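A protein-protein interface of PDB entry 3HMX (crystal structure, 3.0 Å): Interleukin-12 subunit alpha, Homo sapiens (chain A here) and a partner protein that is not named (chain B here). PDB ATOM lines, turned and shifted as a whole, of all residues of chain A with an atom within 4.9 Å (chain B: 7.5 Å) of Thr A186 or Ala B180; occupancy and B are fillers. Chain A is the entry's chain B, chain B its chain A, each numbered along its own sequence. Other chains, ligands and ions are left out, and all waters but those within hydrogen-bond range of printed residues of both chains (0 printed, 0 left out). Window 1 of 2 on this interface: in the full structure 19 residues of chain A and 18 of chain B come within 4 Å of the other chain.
Thr A186 touches two residues of chain B.
Ala B180 touches four residues of chain A.
Of the printed residues of chain B, Leu A64 touches Pro B178 (3.4 Å), Ala B179 (3.6 Å), Ala B180 (3.9 Å) and Tyr B246 (3.6 Å).
Of the printed residues of chain A, Pro B178 touches Glu A61 and Leu A64.
Of the printed residues of chain B, Ile A182 touches Glu B181 (3.0 Å) and Arg B208 (3.7 Å).
Of the printed residues of chain B, Asp A188 touches Tyr B292 (3.4 Å).
Val A190 touches none of the printed residues of chain B.
Cys B177 touches none of the printed residues of chain A.
The nearest residue of chain A that does not touch Ala B180 is Thr A59 (4.6 Å).
The nearest printed residue of chain B that does not touch Val A60 is Pro B178 (4.9 Å).
OE2 of Glu B181 sits at hydrogen-bond distance from OG1 of Thr A186 (2.9 Å).
The backbone carbonyl oxygen of Tyr B246 sits at hydrogen-bond distance from the guanidinium group of Arg A189, 2.9 Å away.
OD2 of Asp A188 sits at hydrogen-bond distance from OH of Tyr B292, 3.4 Å away.
The side-chain hydroxyl (OH) of Tyr B246 sits at hydrogen-bond distance from the backbone carbonyl oxygen (O) of Cys A63 (2.8 Å).
The backbone carbonyl oxygen of Val A60 is in hydrogen-bond range of the backbone NH of Ala B180, 3.0 Å away.
O of Ala B180 is in hydrogen-bond range of OG1 of Thr A186.
The backbone NH (N) of Arg A189 is in hydrogen-bond range of the side-chain hydroxyl (OH) of Tyr B292, 3.3 Å away.
The side-chain carboxylate of Glu B181 is in salt-bridge range of the guanidinium group of Arg A183 (2.5 Å).
The backbone carbonyl oxygen (O) of Ile A182 lies close to the side-chain carboxylate (OE2) of Glu B181 (3.0 Å).
The backbone carbonyl oxygen (O) of Glu B182 is in hydrogen-bond range of the guanidinium group (NH1) of Arg B208, 2.9 Å away.
Ala B179 touches Val A60 (CB to CG2, 3.7 Å).
Val A60 touches Glu B181.
O of Glu A61 touches O of Pro B178, at 3.8 Å.
Cys A63 touches Ala B180.
Leu A64 touches Ala B179 (CD2 to O, 3.6 Å).
Ala B180 touches Leu A64 (CB to CG, 3.9 Å).
Tyr B246 touches Leu A64 (OH to CA, 3.6 Å).
Val A185 touches Tyr B292 (CG1 to CG, 3.5 Å).
CG1 of Val A185 touches OH of Tyr B293, 3.4 Å away.
Arg A189 touches Phe B247 (NE to CD2, 3.8 Å).
Printed residues of chain B that touch a printed residue of chain A: Pro B178, Ala B179, Ala B180, Glu B181, Arg B208, Tyr B246, Phe B247, Tyr B292 and Tyr B293.
Along chain B the printed residues that touch a printed residue of chain A span positions 178 to 293.
Of the 14 printed residues of chain A, 10 touch a printed residue of chain B.
Hydrophobic or aromatic side chains of chain A within 4 Å of the printed part of chain B: Val A60, Leu A64, Ile A182 and Val A185.
Among the printed residues, 21 pairs touch across the chains.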
ATOM      1  N   THR A  59      23.727  -9.284   6.998  1.00  0.00           N
ATOM      2  CA  THR A  59      24.643  -9.040   8.100  1.00  0.00           C
ATOM      3  C   THR A  59      23.944  -8.316   9.248  1.00  0.00           C
ATOM      4  O   THR A  59      24.358  -8.413  10.401  1.00  0.00           O
ATOM      5  CB  THR A  59      25.846  -8.210   7.626  1.00  0.00           C
ATOM      6  OG1 THR A  59      26.569  -7.715   8.757  1.00  0.00           O
ATOM      7  CG2 THR A  59      25.374  -7.039   6.780  1.00  0.00           C
ATOM      8  N   VAL A  60      22.875  -7.594   8.930  1.00  0.00           N
ATOM      9  CA  VAL A  60      22.147  -6.827   9.934  1.00  0.00           C
ATOM     10  C   VAL A  60      21.167  -7.714  10.693  1.00  0.00           C
ATOM     11  O   VAL A  60      21.045  -7.619  11.917  1.00  0.00           O
ATOM     12  CB  VAL A  60      21.392  -5.637   9.302  1.00  0.00           C
ATOM     13  CG1 VAL A  60      20.369  -6.135   8.288  1.00  0.00           C
ATOM     14  CG2 VAL A  60      20.730  -4.793  10.376  1.00  0.00           C
ATOM     15  N   GLU A  61      20.474  -8.579   9.960  1.00  0.00           N
ATOM     16  CA  GLU A  61      19.527  -9.504  10.562  1.00  0.00           C
ATOM     17  C   GLU A  61      20.172 -10.351  11.660  1.00  0.00           C
ATOM     18  O   GLU A  61      19.732 -10.331  12.806  1.00  0.00           O
ATOM     19  CB  GLU A  61      18.919 -10.419   9.495  1.00  0.00           C
ATOM     20  CG  GLU A  61      18.046 -11.535  10.066  1.00  0.00           C
ATOM     21  CD  GLU A  61      17.681 -12.594   9.036  1.00  0.00           C
ATOM     22  OE1 GLU A  61      17.965 -12.384   7.837  1.00  0.00           O
ATOM     23  OE2 GLU A  61      17.112 -13.637   9.426  1.00  0.00           O
ATOM     24  N   CYS A  63      23.509 -10.857  13.348  1.00  0.00           N
ATOM     25  CA  CYS A  63      24.849 -10.673  13.894  1.00  0.00           C
ATOM     26  C   CYS A  63      24.834 -10.326  15.378  1.00  0.00           C
ATOM     27  O   CYS A  63      25.836  -9.867  15.924  1.00  0.00           O
ATOM     28  CB  CYS A  63      25.616  -9.609  13.114  1.00  0.00           C
ATOM     29  SG  CYS A  63      26.520 -10.248  11.697  1.00  0.00           S
ATOM     30  N   LEU A  64      23.695 -10.543  16.027  1.00  0.00           N
ATOM     31  CA  LEU A  64      23.582 -10.313  17.461  1.00  0.00           C
ATOM     32  C   LEU A  64      23.970 -11.588  18.191  1.00  0.00           C
ATOM     33  O   LEU A  64      23.830 -12.678  17.641  1.00  0.00           O
ATOM     34  CB  LEU A  64      22.154  -9.920  17.842  1.00  0.00           C
ATOM     35  CG  LEU A  64      21.286  -9.211  16.804  1.00  0.00           C
ATOM     36  CD1 LEU A  64      20.637 -10.239  15.887  1.00  0.00           C
ATOM     37  CD2 LEU A  64      20.225  -8.362  17.489  1.00  0.00           C
ATOM     38  N   ILE A 182      30.048   2.758  11.187  1.00  0.00           N
ATOM     39  CA  ILE A 182      28.924   2.104  11.847  1.00  0.00           C
ATOM     40  C   ILE A 182      29.010   0.600  11.593  1.00  0.00           C
ATOM     41  O   ILE A 182      28.813  -0.207  12.496  1.00  0.00           O
ATOM     42  CB  ILE A 182      27.561   2.696  11.397  1.00  0.00           C
ATOM     43  CG1 ILE A 182      27.197   3.918  12.250  1.00  0.00           C
ATOM     44  CG2 ILE A 182      26.454   1.675  11.515  1.00  0.00           C
ATOM     45  CD1 ILE A 182      28.064   5.135  12.020  1.00  0.00           C
ATOM     46  N   ARG A 183      29.339   0.224  10.367  1.00  0.00           N
ATOM     47  CA  ARG A 183      29.539  -1.182  10.060  1.00  0.00           C
ATOM     48  C   ARG A 183      30.738  -1.756  10.806  1.00  0.00           C
ATOM     49  O   ARG A 183      30.643  -2.824  11.400  1.00  0.00           O
ATOM     50  CB  ARG A 183      29.717  -1.406   8.565  1.00  0.00           C
ATOM     51  CG  ARG A 183      29.846  -2.861   8.236  1.00  0.00           C
ATOM     52  CD  ARG A 183      28.699  -3.642   8.856  1.00  0.00           C
ATOM     53  NE  ARG A 183      27.700  -3.999   7.858  1.00  0.00           N
ATOM     54  CZ  ARG A 183      26.443  -3.573   7.852  1.00  0.00           C
ATOM     55  NH1 ARG A 183      26.004  -2.768   8.806  1.00  0.00           N
ATOM     56  NH2 ARG A 183      25.623  -3.965   6.890  1.00  0.00           N
ATOM     57  N   ALA A 184      31.868  -1.053  10.765  1.00  0.00           N
ATOM     58  CA  ALA A 184      33.080  -1.506  11.441  1.00  0.00           C
ATOM     59  C   ALA A 184      32.815  -1.739  12.917  1.00  0.00           C
ATOM     60  O   ALA A 184      33.340  -2.680  13.509  1.00  0.00           O
ATOM     61  CB  ALA A 184      34.199  -0.504  11.270  1.00  0.00           C
ATOM     62  N   VAL A 185      32.003  -0.877  13.513  1.00  0.00           N
ATOM     63  CA  VAL A 185      31.630  -1.031  14.909  1.00  0.00           C
ATOM     64  C   VAL A 185      30.937  -2.367  15.139  1.00  0.00           C
ATOM     65  O   VAL A 185      31.325  -3.134  16.022  1.00  0.00           O
ATOM     66  CB  VAL A 185      30.700   0.099  15.370  1.00  0.00           C
ATOM     67  CG1 VAL A 185      29.989  -0.296  16.656  1.00  0.00           C
ATOM     68  CG2 VAL A 185      31.485   1.384  15.554  1.00  0.00           C
ATOM     69  N   THR A 186      29.911  -2.649  14.344  1.00  0.00           N
ATOM     70  CA  THR A 186      29.192  -3.908  14.482  1.00  0.00           C
ATOM     71  C   THR A 186      30.144  -5.083  14.300  1.00  0.00           C
ATOM     72  O   THR A 186      29.982  -6.122  14.938  1.00  0.00           O
ATOM     73  CB  THR A 186      28.019  -4.015  13.493  1.00  0.00           C
ATOM     74  OG1 THR A 186      26.938  -3.190  13.949  1.00  0.00           O
ATOM     75  CG2 THR A 186      27.538  -5.459  13.393  1.00  0.00           C
ATOM     76  N   ILE A 187      31.142  -4.904  13.440  1.00  0.00           N
ATOM     77  CA  ILE A 187      32.186  -5.903  13.271  1.00  0.00           C
ATOM     78  C   ILE A 187      32.938  -6.122  14.578  1.00  0.00           C
ATOM     79  O   ILE A 187      33.021  -7.246  15.076  1.00  0.00           O
ATOM     80  CB  ILE A 187      33.174  -5.512  12.161  1.00  0.00           C
ATOM     81  CG1 ILE A 187      32.639  -5.948  10.801  1.00  0.00           C
ATOM     82  CG2 ILE A 187      34.540  -6.141  12.399  1.00  0.00           C
ATOM     83  CD1 ILE A 187      33.667  -5.865   9.705  1.00  0.00           C
ATOM     84  N   ASP A 188      33.472  -5.045  15.143  1.00  0.00           N
ATOM     85  CA  ASP A 188      34.183  -5.133  16.410  1.00  0.00           C
ATOM     86  C   ASP A 188      33.316  -5.797  17.484  1.00  0.00           C
ATOM     87  O   ASP A 188      33.805  -6.630  18.250  1.00  0.00           O
ATOM     88  CB  ASP A 188      34.654  -3.748  16.856  1.00  0.00           C
ATOM     89  CG  ASP A 188      35.842  -3.807  17.796  1.00  0.00           C
ATOM     90  OD1 ASP A 188      36.860  -3.157  17.487  1.00  0.00           O
ATOM     91  OD2 ASP A 188      35.760  -4.498  18.835  1.00  0.00           O
ATOM     92  N   ARG A 189      32.033  -5.441  17.524  1.00  0.00           N
ATOM     93  CA  ARG A 189      31.093  -6.047  18.470  1.00  0.00           C
ATOM     94  C   ARG A 189      31.101  -7.570  18.407  1.00  0.00           C
ATOM     95  O   ARG A 189      31.089  -8.240  19.437  1.00  0.00           O
ATOM     96  CB  ARG A 189      29.671  -5.539  18.225  1.00  0.00           C
ATOM     97  CG  ARG A 189      29.374  -4.208  18.874  1.00  0.00           C
ATOM     98  CD  ARG A 189      27.875  -3.975  19.026  1.00  0.00           C
ATOM     99  NE  ARG A 189      27.614  -3.010  20.087  1.00  0.00           N
ATOM    100  CZ  ARG A 189      27.585  -1.695  19.910  1.00  0.00           C
ATOM    101  NH1 ARG A 189      27.782  -1.184  18.706  1.00  0.00           N
ATOM    102  NH2 ARG A 189      27.352  -0.888  20.936  1.00  0.00           N
ATOM    103  N   VAL A 190      31.107  -8.111  17.194  1.00  0.00           N
ATOM    104  CA  VAL A 190      31.131  -9.553  17.010  1.00  0.00           C
ATOM    105  C   VAL A 190      32.471 -10.118  17.459  1.00  0.00           C
ATOM    106  O   VAL A 190      32.527 -11.059  18.246  1.00  0.00           O
ATOM    107  CB  VAL A 190      30.883  -9.936  15.542  1.00  0.00           C
ATOM    108  CG1 VAL A 190      30.948 -11.443  15.368  1.00  0.00           C
ATOM    109  CG2 VAL A 190      29.534  -9.394  15.078  1.00  0.00           C
ATOM    110  N   CYS B 177      11.828  -8.867  15.343  1.00  0.00           N
ATOM    111  CA  CYS B 177      13.157  -9.415  15.108  1.00  0.00           C
ATOM    112  C   CYS B 177      14.196  -8.305  15.228  1.00  0.00           C
ATOM    113  O   CYS B 177      14.325  -7.470  14.332  1.00  0.00           O
ATOM    114  CB  CYS B 177      13.236 -10.071  13.731  1.00  0.00           C
ATOM    115  SG  CYS B 177      12.234 -11.561  13.549  1.00  0.00           S
ATOM    116  N   PRO B 178      14.933  -8.286  16.348  1.00  0.00           N
ATOM    117  CA  PRO B 178      15.937  -7.254  16.628  1.00  0.00           C
ATOM    118  C   PRO B 178      17.109  -7.288  15.647  1.00  0.00           C
ATOM    119  O   PRO B 178      17.604  -8.361  15.300  1.00  0.00           O
ATOM    120  CB  PRO B 178      16.414  -7.604  18.041  1.00  0.00           C
ATOM    121  CG  PRO B 178      15.315  -8.428  18.629  1.00  0.00           C
ATOM    122  CD  PRO B 178      14.777  -9.217  17.478  1.00  0.00           C
ATOM    123  N   ALA B 179      17.542  -6.109  15.211  1.00  0.00           N
ATOM    124  CA  ALA B 179      18.652  -5.983  14.277  1.00  0.00           C
ATOM    125  C   ALA B 179      19.945  -5.643  15.017  1.00  0.00           C
ATOM    126  O   ALA B 179      19.912  -5.058  16.097  1.00  0.00           O
ATOM    127  CB  ALA B 179      18.336  -4.922  13.234  1.00  0.00           C
ATOM    128  N   ALA B 180      21.081  -6.009  14.431  1.00  0.00           N
ATOM    129  CA  ALA B 180      22.377  -5.780  15.067  1.00  0.00           C
ATOM    130  C   ALA B 180      22.889  -4.364  14.849  1.00  0.00           C
ATOM    131  O   ALA B 180      24.015  -4.036  15.230  1.00  0.00           O
ATOM    132  CB  ALA B 180      23.395  -6.789  14.555  1.00  0.00           C
ATOM    133  N   GLU B 181      22.048  -3.525  14.251  1.00  0.00           N
ATOM    134  CA  GLU B 181      22.465  -2.206  13.797  1.00  0.00           C
ATOM    135  C   GLU B 181      21.253  -1.423  13.300  1.00  0.00           C
ATOM    136  O   GLU B 181      20.393  -1.974  12.610  1.00  0.00           O
ATOM    137  CB  GLU B 181      23.468  -2.368  12.659  1.00  0.00           C
ATOM    138  CG  GLU B 181      24.505  -1.272  12.554  1.00  0.00           C
ATOM    139  CD  GLU B 181      25.352  -1.415  11.303  1.00  0.00           C
ATOM    140  OE1 GLU B 181      24.840  -1.083  10.213  1.00  0.00           O
ATOM    141  OE2 GLU B 181      26.522  -1.852  11.405  1.00  0.00           O
ATOM    142  N   GLU B 182      21.190  -0.139  13.642  1.00  0.00           N
ATOM    143  CA  GLU B 182      20.068   0.711  13.255  1.00  0.00           C
ATOM    144  C   GLU B 182      20.298   1.346  11.891  1.00  0.00           C
ATOM    145  O   GLU B 182      21.243   2.113  11.703  1.00  0.00           O
ATOM    146  CB  GLU B 182      19.878   1.823  14.277  1.00  0.00           C
ATOM    147  CG  GLU B 182      19.560   1.357  15.671  1.00  0.00           C
ATOM    148  CD  GLU B 182      19.729   2.468  16.680  1.00  0.00           C
ATOM    149  OE1 GLU B 182      18.717   3.110  17.032  1.00  0.00           O
ATOM    150  OE2 GLU B 182      20.878   2.713  17.101  1.00  0.00           O
ATOM    151  N   ARG B 208      21.777   4.772  19.183  1.00  0.00           N
ATOM    152  CA  ARG B 208      23.226   4.782  19.303  1.00  0.00           C
ATOM    153  C   ARG B 208      23.780   6.182  19.532  1.00  0.00           C
ATOM    154  O   ARG B 208      24.948   6.344  19.862  1.00  0.00           O
ATOM    155  CB  ARG B 208      23.866   4.165  18.059  1.00  0.00           C
ATOM    156  CG  ARG B 208      23.641   4.936  16.763  1.00  0.00           C
ATOM    157  CD  ARG B 208      24.597   4.446  15.671  1.00  0.00           C
ATOM    158  NE  ARG B 208      24.287   4.993  14.351  1.00  0.00           N
ATOM    159  CZ  ARG B 208      23.558   4.361  13.437  1.00  0.00           C
ATOM    160  NH1 ARG B 208      23.063   3.158  13.705  1.00  0.00           N
ATOM    161  NH2 ARG B 208      23.320   4.930  12.259  1.00  0.00           N
ATOM    162  N   TYR B 246      29.857  -7.762  23.870  1.00  0.00           N
ATOM    163  CA  TYR B 246      29.241  -7.339  22.627  1.00  0.00           C
ATOM    164  C   TYR B 246      28.836  -5.883  22.758  1.00  0.00           C
ATOM    165  O   TYR B 246      28.626  -5.191  21.767  1.00  0.00           O
ATOM    166  CB  TYR B 246      28.011  -8.197  22.351  1.00  0.00           C
ATOM    167  CG  TYR B 246      27.395  -7.975  20.996  1.00  0.00           C
ATOM    168  CD1 TYR B 246      26.299  -7.148  20.839  1.00  0.00           C
ATOM    169  CD2 TYR B 246      27.911  -8.595  19.870  1.00  0.00           C
ATOM    170  CE1 TYR B 246      25.728  -6.944  19.600  1.00  0.00           C
ATOM    171  CE2 TYR B 246      27.347  -8.397  18.625  1.00  0.00           C
ATOM    172  CZ  TYR B 246      26.256  -7.571  18.497  1.00  0.00           C
ATOM    173  OH  TYR B 246      25.692  -7.372  17.260  1.00  0.00           O
ATOM    174  N   PHE B 247      28.727  -5.430  24.003  1.00  0.00           N
ATOM    175  CA  PHE B 247      28.338  -4.064  24.316  1.00  0.00           C
ATOM    176  C   PHE B 247      29.370  -3.433  25.231  1.00  0.00           C
ATOM    177  O   PHE B 247      29.076  -3.106  26.379  1.00  0.00           O
ATOM    178  CB  PHE B 247      26.990  -4.047  25.025  1.00  0.00           C
ATOM    179  CG  PHE B 247      25.843  -4.481  24.165  1.00  0.00           C
ATOM    180  CD1 PHE B 247      25.192  -5.673  24.412  1.00  0.00           C
ATOM    181  CD2 PHE B 247      25.404  -3.691  23.119  1.00  0.00           C
ATOM    182  CE1 PHE B 247      24.128  -6.070  23.630  1.00  0.00           C
ATOM    183  CE2 PHE B 247      24.344  -4.087  22.333  1.00  0.00           C
ATOM    184  CZ  PHE B 247      23.706  -5.276  22.588  1.00  0.00           C
ATOM    185  N   TYR B 292      31.965   2.390  21.789  1.00  0.00           N
ATOM    186  CA  TYR B 292      32.037   2.614  20.354  1.00  0.00           C
ATOM    187  C   TYR B 292      31.793   4.059  19.911  1.00  0.00           C
ATOM    188  O   TYR B 292      32.590   4.612  19.161  1.00  0.00           O
ATOM    189  CB  TYR B 292      31.125   1.635  19.612  1.00  0.00           C
ATOM    190  CG  TYR B 292      31.562   0.194  19.779  1.00  0.00           C
ATOM    191  CD1 TYR B 292      30.792  -0.711  20.498  1.00  0.00           C
ATOM    192  CD2 TYR B 292      32.761  -0.256  19.234  1.00  0.00           C
ATOM    193  CE1 TYR B 292      31.195  -2.027  20.656  1.00  0.00           C
ATOM    194  CE2 TYR B 292      33.170  -1.570  19.388  1.00  0.00           C
ATOM    195  CZ  TYR B 292      32.383  -2.450  20.100  1.00  0.00           C
ATOM    196  OH  TYR B 292      32.787  -3.758  20.257  1.00  0.00           O
ATOM    197  N   TYR B 293      30.708   4.672  20.375  1.00  0.00           N
ATOM    198  CA  TYR B 293      30.353   6.019  19.926  1.00  0.00           C
ATOM    199  C   TYR B 293      30.614   7.079  20.995  1.00  0.00           C
ATOM    200  O   TYR B 293      30.571   6.787  22.183  1.00  0.00           O
ATOM    201  CB  TYR B 293      28.890   6.059  19.486  1.00  0.00           C
ATOM    202  CG  TYR B 293      28.514   4.949  18.533  1.00  0.00           C
ATOM    203  CD1 TYR B 293      28.965   4.947  17.221  1.00  0.00           C
ATOM    204  CD2 TYR B 293      27.708   3.905  18.946  1.00  0.00           C
ATOM    205  CE1 TYR B 293      28.622   3.930  16.348  1.00  0.00           C
ATOM    206  CE2 TYR B 293      27.357   2.883  18.079  1.00  0.00           C
ATOM    207  CZ  TYR B 293      27.815   2.899  16.783  1.00  0.00           C
ATOM    208  OH  TYR B 293      27.467   1.881  15.917  1.00  0.00           O
